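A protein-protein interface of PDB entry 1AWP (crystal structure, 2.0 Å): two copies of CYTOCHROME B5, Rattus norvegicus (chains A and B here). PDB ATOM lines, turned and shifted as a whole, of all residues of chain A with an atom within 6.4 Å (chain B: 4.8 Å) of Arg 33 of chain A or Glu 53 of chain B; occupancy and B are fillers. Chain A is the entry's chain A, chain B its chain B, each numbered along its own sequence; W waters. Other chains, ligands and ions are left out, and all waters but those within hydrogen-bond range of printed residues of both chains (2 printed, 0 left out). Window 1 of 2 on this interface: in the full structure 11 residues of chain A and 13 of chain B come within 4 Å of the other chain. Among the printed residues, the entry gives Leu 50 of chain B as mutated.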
ATOM      1  N   MET A  28     -24.739   6.730  -9.072  1.00  0.00           N
ATOM      2  CA  MET A  28     -24.518   7.759 -10.063  1.00  0.00           C
ATOM      3  C   MET A  28     -23.453   8.701  -9.519  1.00  0.00           C
ATOM      4  O   MET A  28     -23.395   8.947  -8.314  1.00  0.00           O
ATOM      5  CB  MET A  28     -25.834   8.506 -10.283  1.00  0.00           C
ATOM      6  CG  MET A  28     -25.772   9.670 -11.244  1.00  0.00           C
ATOM      7  SD  MET A  28     -27.429  10.313 -11.504  1.00  0.00           S
ATOM      8  CE  MET A  28     -28.045   9.161 -12.703  1.00  0.00           C
ATOM      9  N   VAL A  29     -22.596   9.207 -10.400  1.00  0.00           N
ATOM     10  CA  VAL A  29     -21.552  10.135  -9.986  1.00  0.00           C
ATOM     11  C   VAL A  29     -21.948  11.558 -10.397  1.00  0.00           C
ATOM     12  O   VAL A  29     -22.382  11.793 -11.528  1.00  0.00           O
ATOM     13  CB  VAL A  29     -20.180   9.763 -10.625  1.00  0.00           C
ATOM     14  CG1 VAL A  29     -19.211  10.920 -10.520  1.00  0.00           C
ATOM     15  CG2 VAL A  29     -19.598   8.555  -9.916  1.00  0.00           C
ATOM     16  N   ILE A  30     -21.821  12.493  -9.459  1.00  0.00           N
ATOM     17  CA  ILE A  30     -22.137  13.900  -9.706  1.00  0.00           C
ATOM     18  C   ILE A  30     -21.067  14.736  -9.002  1.00  0.00           C
ATOM     19  O   ILE A  30     -20.902  14.651  -7.787  1.00  0.00           O
ATOM     20  CB  ILE A  30     -23.547  14.257  -9.169  1.00  0.00           C
ATOM     21  CG1 ILE A  30     -24.604  13.561 -10.027  1.00  0.00           C
ATOM     22  CG2 ILE A  30     -23.778  15.760  -9.233  1.00  0.00           C
ATOM     23  CD1 ILE A  30     -26.017  13.901  -9.655  1.00  0.00           C
ATOM     24  N   HIS A  31     -20.320  15.516  -9.778  1.00  0.00           N
ATOM     25  CA  HIS A  31     -19.259  16.352  -9.226  1.00  0.00           C
ATOM     26  C   HIS A  31     -18.261  15.585  -8.352  1.00  0.00           C
ATOM     27  O   HIS A  31     -17.900  16.033  -7.259  1.00  0.00           O
ATOM     28  CB  HIS A  31     -19.857  17.505  -8.425  1.00  0.00           C
ATOM     29  CG  HIS A  31     -20.472  18.567  -9.277  1.00  0.00           C
ATOM     30  ND1 HIS A  31     -19.753  19.269 -10.223  1.00  0.00           N
ATOM     31  CD2 HIS A  31     -21.737  19.044  -9.337  1.00  0.00           C
ATOM     32  CE1 HIS A  31     -20.551  20.129 -10.829  1.00  0.00           C
ATOM     33  NE2 HIS A  31     -21.761  20.013 -10.308  1.00  0.00           N
ATOM     34  N   GLY A  32     -17.835  14.421  -8.833  1.00  0.00           N
ATOM     35  CA  GLY A  32     -16.852  13.623  -8.115  1.00  0.00           C
ATOM     36  C   GLY A  32     -17.310  12.877  -6.881  1.00  0.00           C
ATOM     37  O   GLY A  32     -16.486  12.306  -6.173  1.00  0.00           O
ATOM     38  N   ARG A  33     -18.611  12.875  -6.612  1.00  0.00           N
ATOM     39  CA  ARG A  33     -19.131  12.170  -5.446  1.00  0.00           C
ATOM     40  C   ARG A  33     -20.094  11.072  -5.886  1.00  0.00           C
ATOM     41  O   ARG A  33     -20.769  11.199  -6.911  1.00  0.00           O
ATOM     42  CB  ARG A  33     -19.819  13.159  -4.497  1.00  0.00           C
ATOM     43  CG  ARG A  33     -18.826  13.864  -3.584  1.00  0.00           C
ATOM     44  CD  ARG A  33     -19.442  14.993  -2.769  1.00  0.00           C
ATOM     45  NE  ARG A  33     -18.470  15.527  -1.819  1.00  0.00           N
ATOM     46  CZ  ARG A  33     -18.736  15.825  -0.550  1.00  0.00           C
ATOM     47  NH1 ARG A  33     -19.949  15.647  -0.058  1.00  0.00           N
ATOM     48  NH2 ARG A  33     -17.776  16.277   0.238  1.00  0.00           N
ATOM     49  N   VAL A  34     -20.148   9.993  -5.117  1.00  0.00           N
ATOM     50  CA  VAL A  34     -21.009   8.868  -5.457  1.00  0.00           C
ATOM     51  C   VAL A  34     -22.314   8.927  -4.685  1.00  0.00           C
ATOM     52  O   VAL A  34     -22.316   9.200  -3.483  1.00  0.00           O
ATOM     53  CB  VAL A  34     -20.299   7.520  -5.162  1.00  0.00           C
ATOM     54  CG1 VAL A  34     -21.172   6.350  -5.622  1.00  0.00           C
ATOM     55  CG2 VAL A  34     -18.944   7.482  -5.873  1.00  0.00           C
ATOM     56  N   TYR A  35     -23.421   8.671  -5.383  1.00  0.00           N
ATOM     57  CA  TYR A  35     -24.747   8.697  -4.777  1.00  0.00           C
ATOM     58  C   TYR A  35     -25.524   7.437  -5.091  1.00  0.00           C
ATOM     59  O   TYR A  35     -25.581   6.995  -6.234  1.00  0.00           O
ATOM     60  CB  TYR A  35     -25.554   9.896  -5.289  1.00  0.00           C
ATOM     61  CG  TYR A  35     -24.922  11.229  -4.992  1.00  0.00           C
ATOM     62  CD1 TYR A  35     -24.014  11.806  -5.879  1.00  0.00           C
ATOM     63  CD2 TYR A  35     -25.200  11.897  -3.804  1.00  0.00           C
ATOM     64  CE1 TYR A  35     -23.397  13.012  -5.585  1.00  0.00           C
ATOM     65  CE2 TYR A  35     -24.587  13.106  -3.497  1.00  0.00           C
ATOM     66  CZ  TYR A  35     -23.685  13.657  -4.389  1.00  0.00           C
ATOM     67  OH  TYR A  35     -23.062  14.844  -4.067  1.00  0.00           O
ATOM     68  N   LYS A  77     -27.821  15.327  -0.706  1.00  0.00           N
ATOM     69  CA  LYS A  77     -27.206  14.995   0.558  1.00  0.00           C
ATOM     70  C   LYS A  77     -27.650  13.680   1.184  1.00  0.00           C
ATOM     71  O   LYS A  77     -26.858  13.042   1.876  1.00  0.00           O
ATOM     72  CB  LYS A  77     -27.417  16.134   1.550  1.00  0.00           C
ATOM     73  CG  LYS A  77     -26.177  16.976   1.758  1.00  0.00           C
ATOM     74  CD  LYS A  77     -26.454  18.451   1.520  1.00  0.00           C
ATOM     75  CE  LYS A  77     -27.183  19.065   2.696  1.00  0.00           C
ATOM     76  NZ  LYS A  77     -27.001  20.532   2.712  1.00  0.00           N
ATOM     77  N   TYR A  80     -25.677  10.544  -0.653  1.00  0.00           N
ATOM     78  CA  TYR A  80     -24.221  10.529  -0.659  1.00  0.00           C
ATOM     79  C   TYR A  80     -23.640   9.319   0.072  1.00  0.00           C
ATOM     80  O   TYR A  80     -23.932   9.113   1.248  1.00  0.00           O
ATOM     81  CB  TYR A  80     -23.704  11.806  -0.002  1.00  0.00           C
ATOM     82  CG  TYR A  80     -22.204  11.838   0.196  1.00  0.00           C
ATOM     83  CD1 TYR A  80     -21.333  11.775  -0.893  1.00  0.00           C
ATOM     84  CD2 TYR A  80     -21.653  11.966   1.473  1.00  0.00           C
ATOM     85  CE1 TYR A  80     -19.956  11.845  -0.714  1.00  0.00           C
ATOM     86  CE2 TYR A  80     -20.278  12.036   1.660  1.00  0.00           C
ATOM     87  CZ  TYR A  80     -19.439  11.978   0.566  1.00  0.00           C
ATOM     88  OH  TYR A  80     -18.084  12.076   0.752  1.00  0.00           O
ATOM     89  N   GLY A  82     -20.060   8.286  -0.728  1.00  0.00           N
ATOM     90  CA  GLY A  82     -18.608   8.301  -0.796  1.00  0.00           C
ATOM     91  C   GLY A  82     -18.074   9.151  -1.927  1.00  0.00           C
ATOM     92  O   GLY A  82     -18.853   9.725  -2.690  1.00  0.00           O
ATOM     93  N   ASP A  83     -16.747   9.228  -2.034  1.00  0.00           N
ATOM     94  CA  ASP A  83     -16.074  10.016  -3.071  1.00  0.00           C
ATOM     95  C   ASP A  83     -15.420   9.138  -4.143  1.00  0.00           C
ATOM     96  O   ASP A  83     -15.083   7.975  -3.896  1.00  0.00           O
ATOM     97  CB  ASP A  83     -14.975  10.886  -2.456  1.00  0.00           C
ATOM     98  CG  ASP A  83     -15.512  12.013  -1.596  1.00  0.00           C
ATOM     99  OD1 ASP A  83     -16.744  12.105  -1.404  1.00  0.00           O
ATOM    100  OD2 ASP A  83     -14.685  12.813  -1.111  1.00  0.00           O
ATOM    101  N   VAL A  84     -15.237   9.702  -5.331  1.00  0.00           N
ATOM    102  CA  VAL A  84     -14.584   8.969  -6.406  1.00  0.00           C
ATOM    103  C   VAL A  84     -13.083   9.076  -6.140  1.00  0.00           C
ATOM    104  O   VAL A  84     -12.578  10.139  -5.776  1.00  0.00           O
ATOM    105  CB  VAL A  84     -14.907   9.575  -7.804  1.00  0.00           C
ATOM    106  CG1 VAL A  84     -14.082   8.886  -8.884  1.00  0.00           C
ATOM    107  CG2 VAL A  84     -16.382   9.417  -8.110  1.00  0.00           C
ATOM    108  N   ASN B  21     -15.402  20.627  -3.447  1.00  0.00           N
ATOM    109  CA  ASN B  21     -15.888  19.716  -2.419  1.00  0.00           C
ATOM    110  C   ASN B  21     -14.888  18.741  -1.824  1.00  0.00           C
ATOM    111  O   ASN B  21     -15.261  17.631  -1.454  1.00  0.00           O
ATOM    112  CB  ASN B  21     -17.082  18.927  -2.960  1.00  0.00           C
ATOM    113  CG  ASN B  21     -16.730  18.086  -4.175  1.00  0.00           C
ATOM    114  OD1 ASN B  21     -17.573  17.362  -4.709  1.00  0.00           O
ATOM    115  ND2 ASN B  21     -15.484  18.181  -4.620  1.00  0.00           N
ATOM    116  N   GLU B  49     -14.811  15.966   9.651  1.00  0.00           N
ATOM    117  CA  GLU B  49     -15.606  14.993   8.906  1.00  0.00           C
ATOM    118  C   GLU B  49     -16.994  15.581   8.627  1.00  0.00           C
ATOM    119  O   GLU B  49     -17.538  15.447   7.527  1.00  0.00           O
ATOM    120  CB  GLU B  49     -15.721  13.685   9.702  1.00  0.00           C
ATOM    121  CG  GLU B  49     -14.374  13.038  10.048  1.00  0.00           C
ATOM    122  CD  GLU B  49     -13.806  13.514  11.391  1.00  0.00           C
ATOM    123  OE1 GLU B  49     -14.178  12.943  12.442  1.00  0.00           O
ATOM    124  OE2 GLU B  49     -12.984  14.459  11.402  1.00  0.00           O
ATOM    125  N   LEU B  50     -17.550  16.242   9.638  1.00  0.00           N
ATOM    126  CA  LEU B  50     -18.861  16.875   9.543  1.00  0.00           C
ATOM    127  C   LEU B  50     -18.883  17.948   8.454  1.00  0.00           C
ATOM    128  O   LEU B  50     -19.863  18.076   7.717  1.00  0.00           O
ATOM    129  CB  LEU B  50     -19.215  17.505  10.885  1.00  0.00           C
ATOM    130  CG  LEU B  50     -19.888  16.589  11.895  1.00  0.00           C
ATOM    131  CD1 LEU B  50     -20.447  17.437  13.025  1.00  0.00           C
ATOM    132  CD2 LEU B  50     -20.990  15.792  11.222  1.00  0.00           C
ATOM    133  N   LEU B  51     -17.794  18.714   8.373  1.00  0.00           N
ATOM    134  CA  LEU B  51     -17.640  19.779   7.391  1.00  0.00           C
ATOM    135  C   LEU B  51     -17.473  19.225   5.976  1.00  0.00           C
ATOM    136  O   LEU B  51     -18.208  19.609   5.067  1.00  0.00           O
ATOM    137  CB  LEU B  51     -16.424  20.644   7.734  1.00  0.00           C
ATOM    138  CG  LEU B  51     -16.453  21.463   9.027  1.00  0.00           C
ATOM    139  CD1 LEU B  51     -15.210  22.337   9.110  1.00  0.00           C
ATOM    140  CD2 LEU B  51     -17.689  22.320   9.059  1.00  0.00           C
ATOM    141  N   LEU B  52     -16.508  18.327   5.789  1.00  0.00           N
ATOM    142  CA  LEU B  52     -16.254  17.742   4.475  1.00  0.00           C
ATOM    143  C   LEU B  52     -17.501  17.094   3.892  1.00  0.00           C
ATOM    144  O   LEU B  52     -17.718  17.115   2.683  1.00  0.00           O
ATOM    145  CB  LEU B  52     -15.137  16.705   4.564  1.00  0.00           C
ATOM    146  CG  LEU B  52     -13.727  17.278   4.724  1.00  0.00           C
ATOM    147  CD1 LEU B  52     -12.752  16.134   4.824  1.00  0.00           C
ATOM    148  CD2 LEU B  52     -13.369  18.174   3.550  1.00  0.00           C
ATOM    149  N   GLU B  53     -18.332  16.526   4.750  1.00  0.00           N
ATOM    150  CA  GLU B  53     -19.536  15.881   4.273  1.00  0.00           C
ATOM    151  C   GLU B  53     -20.439  16.862   3.524  1.00  0.00           C
ATOM    152  O   GLU B  53     -21.170  16.476   2.603  1.00  0.00           O
ATOM    153  CB  GLU B  53     -20.295  15.269   5.447  1.00  0.00           C
ATOM    154  CG  GLU B  53     -21.713  14.876   5.107  1.00  0.00           C
ATOM    155  CD  GLU B  53     -22.262  13.811   6.027  1.00  0.00           C
ATOM    156  OE1 GLU B  53     -22.019  13.895   7.248  1.00  0.00           O
ATOM    157  OE2 GLU B  53     -22.941  12.890   5.523  1.00  0.00           O
ATOM    158  N   GLN B  54     -20.385  18.132   3.911  1.00  0.00           N
ATOM    159  CA  GLN B  54     -21.227  19.131   3.274  1.00  0.00           C
ATOM    160  C   GLN B  54     -20.479  20.189   2.489  1.00  0.00           C
ATOM    161  O   GLN B  54     -20.996  21.276   2.250  1.00  0.00           O
ATOM    162  CB  GLN B  54     -22.134  19.771   4.327  1.00  0.00           C
ATOM    163  CG  GLN B  54     -23.226  18.805   4.758  1.00  0.00           C
ATOM    164  CD  GLN B  54     -24.296  19.440   5.593  1.00  0.00           C
ATOM    165  OE1 GLN B  54     -24.396  19.173   6.781  1.00  0.00           O
ATOM    166  NE2 GLN B  54     -25.111  20.280   4.978  1.00  0.00           N
ATOM    167  N   ALA B  55     -19.262  19.865   2.074  1.00  0.00           N
ATOM    168  CA  ALA B  55     -18.469  20.799   1.291  1.00  0.00           C
ATOM    169  C   ALA B  55     -19.111  20.866  -0.083  1.00  0.00           C
ATOM    170  O   ALA B  55     -19.619  19.860  -0.577  1.00  0.00           O
ATOM    171  CB  ALA B  55     -17.042  20.302   1.174  1.00  0.00           C
HETATM  172  O   HOH W   1     -27.461  21.368   6.027  1.00  0.00           O
HETATM  173  O   HOH W   2     -15.706  15.222  -2.749  1.00  0.00           O
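The side-chain amino group of Lys 77 of chain A sits close to the side-chain amide nitrogen of Gln 54 of chain B, 3.0 Å away. The guanidinium group (NH1) of Arg 33 of chain A lies within hydrogen-bond range of the backbone carbonyl oxygen (O) of Glu 53 of chain B, 3.0 Å away. The backbone carbonyl oxygen (O) of His 31 of chain A lies close to the side-chain amide oxygen (OD1) of Asn 21 of chain B, 2.9 Å away. The guanidinium group of Arg 33 of chain A is in hydrogen-bond range of the backbone carbonyl oxygen of Leu 52 of chain B, 2.6 Å away. The guanidinium group of Arg 33 of chain A is in hydrogen-bond range of the backbone carbonyl oxygen of Asn 21 of chain B, 3.3 Å away.
Water W2 lies within hydrogen-bond range of O of Asn 21 of chain B (2.8 Å), NE of Arg 33 of chain A (2.9 Å) and OD2 of Asp 83 of chain A (3.1 Å). Water W1 lies within hydrogen-bond range of NE2 of Gln 54 of chain B (2.8 Å) and NZ of Lys 77 of chain A (3.4 Å).
OD1 of Asp 83 of chain A is in salt-bridge range of NE of Arg 33 of chain A (3.9 Å).
Of the 8 printed residues of chain B, 4 touch a printed residue of chain A.
Of the printed residues of chain B, His 31 of chain A touches Asn 21. Printed residues of chain B within 4 Å of Lys 77 of chain A: Gln 54. Val 84 of chain A touches none of the printed residues of chain B. Printed residues of chain A within 4 Å of Asn 21 of chain B: His 31 and Arg 33. Of the printed residues of chain A, Leu 52 of chain B touches Arg 33. Glu 53 of chain B touches one residue of chain A. Printed residues of chain A within 4 Å of Gln 54 of chain B: Lys 77 (3.0 Å). The nearest residue of chain B that does not touch Arg 33 of chain A is Ala 55 of chain B (4.1 Å).
No position is printed for both chains.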
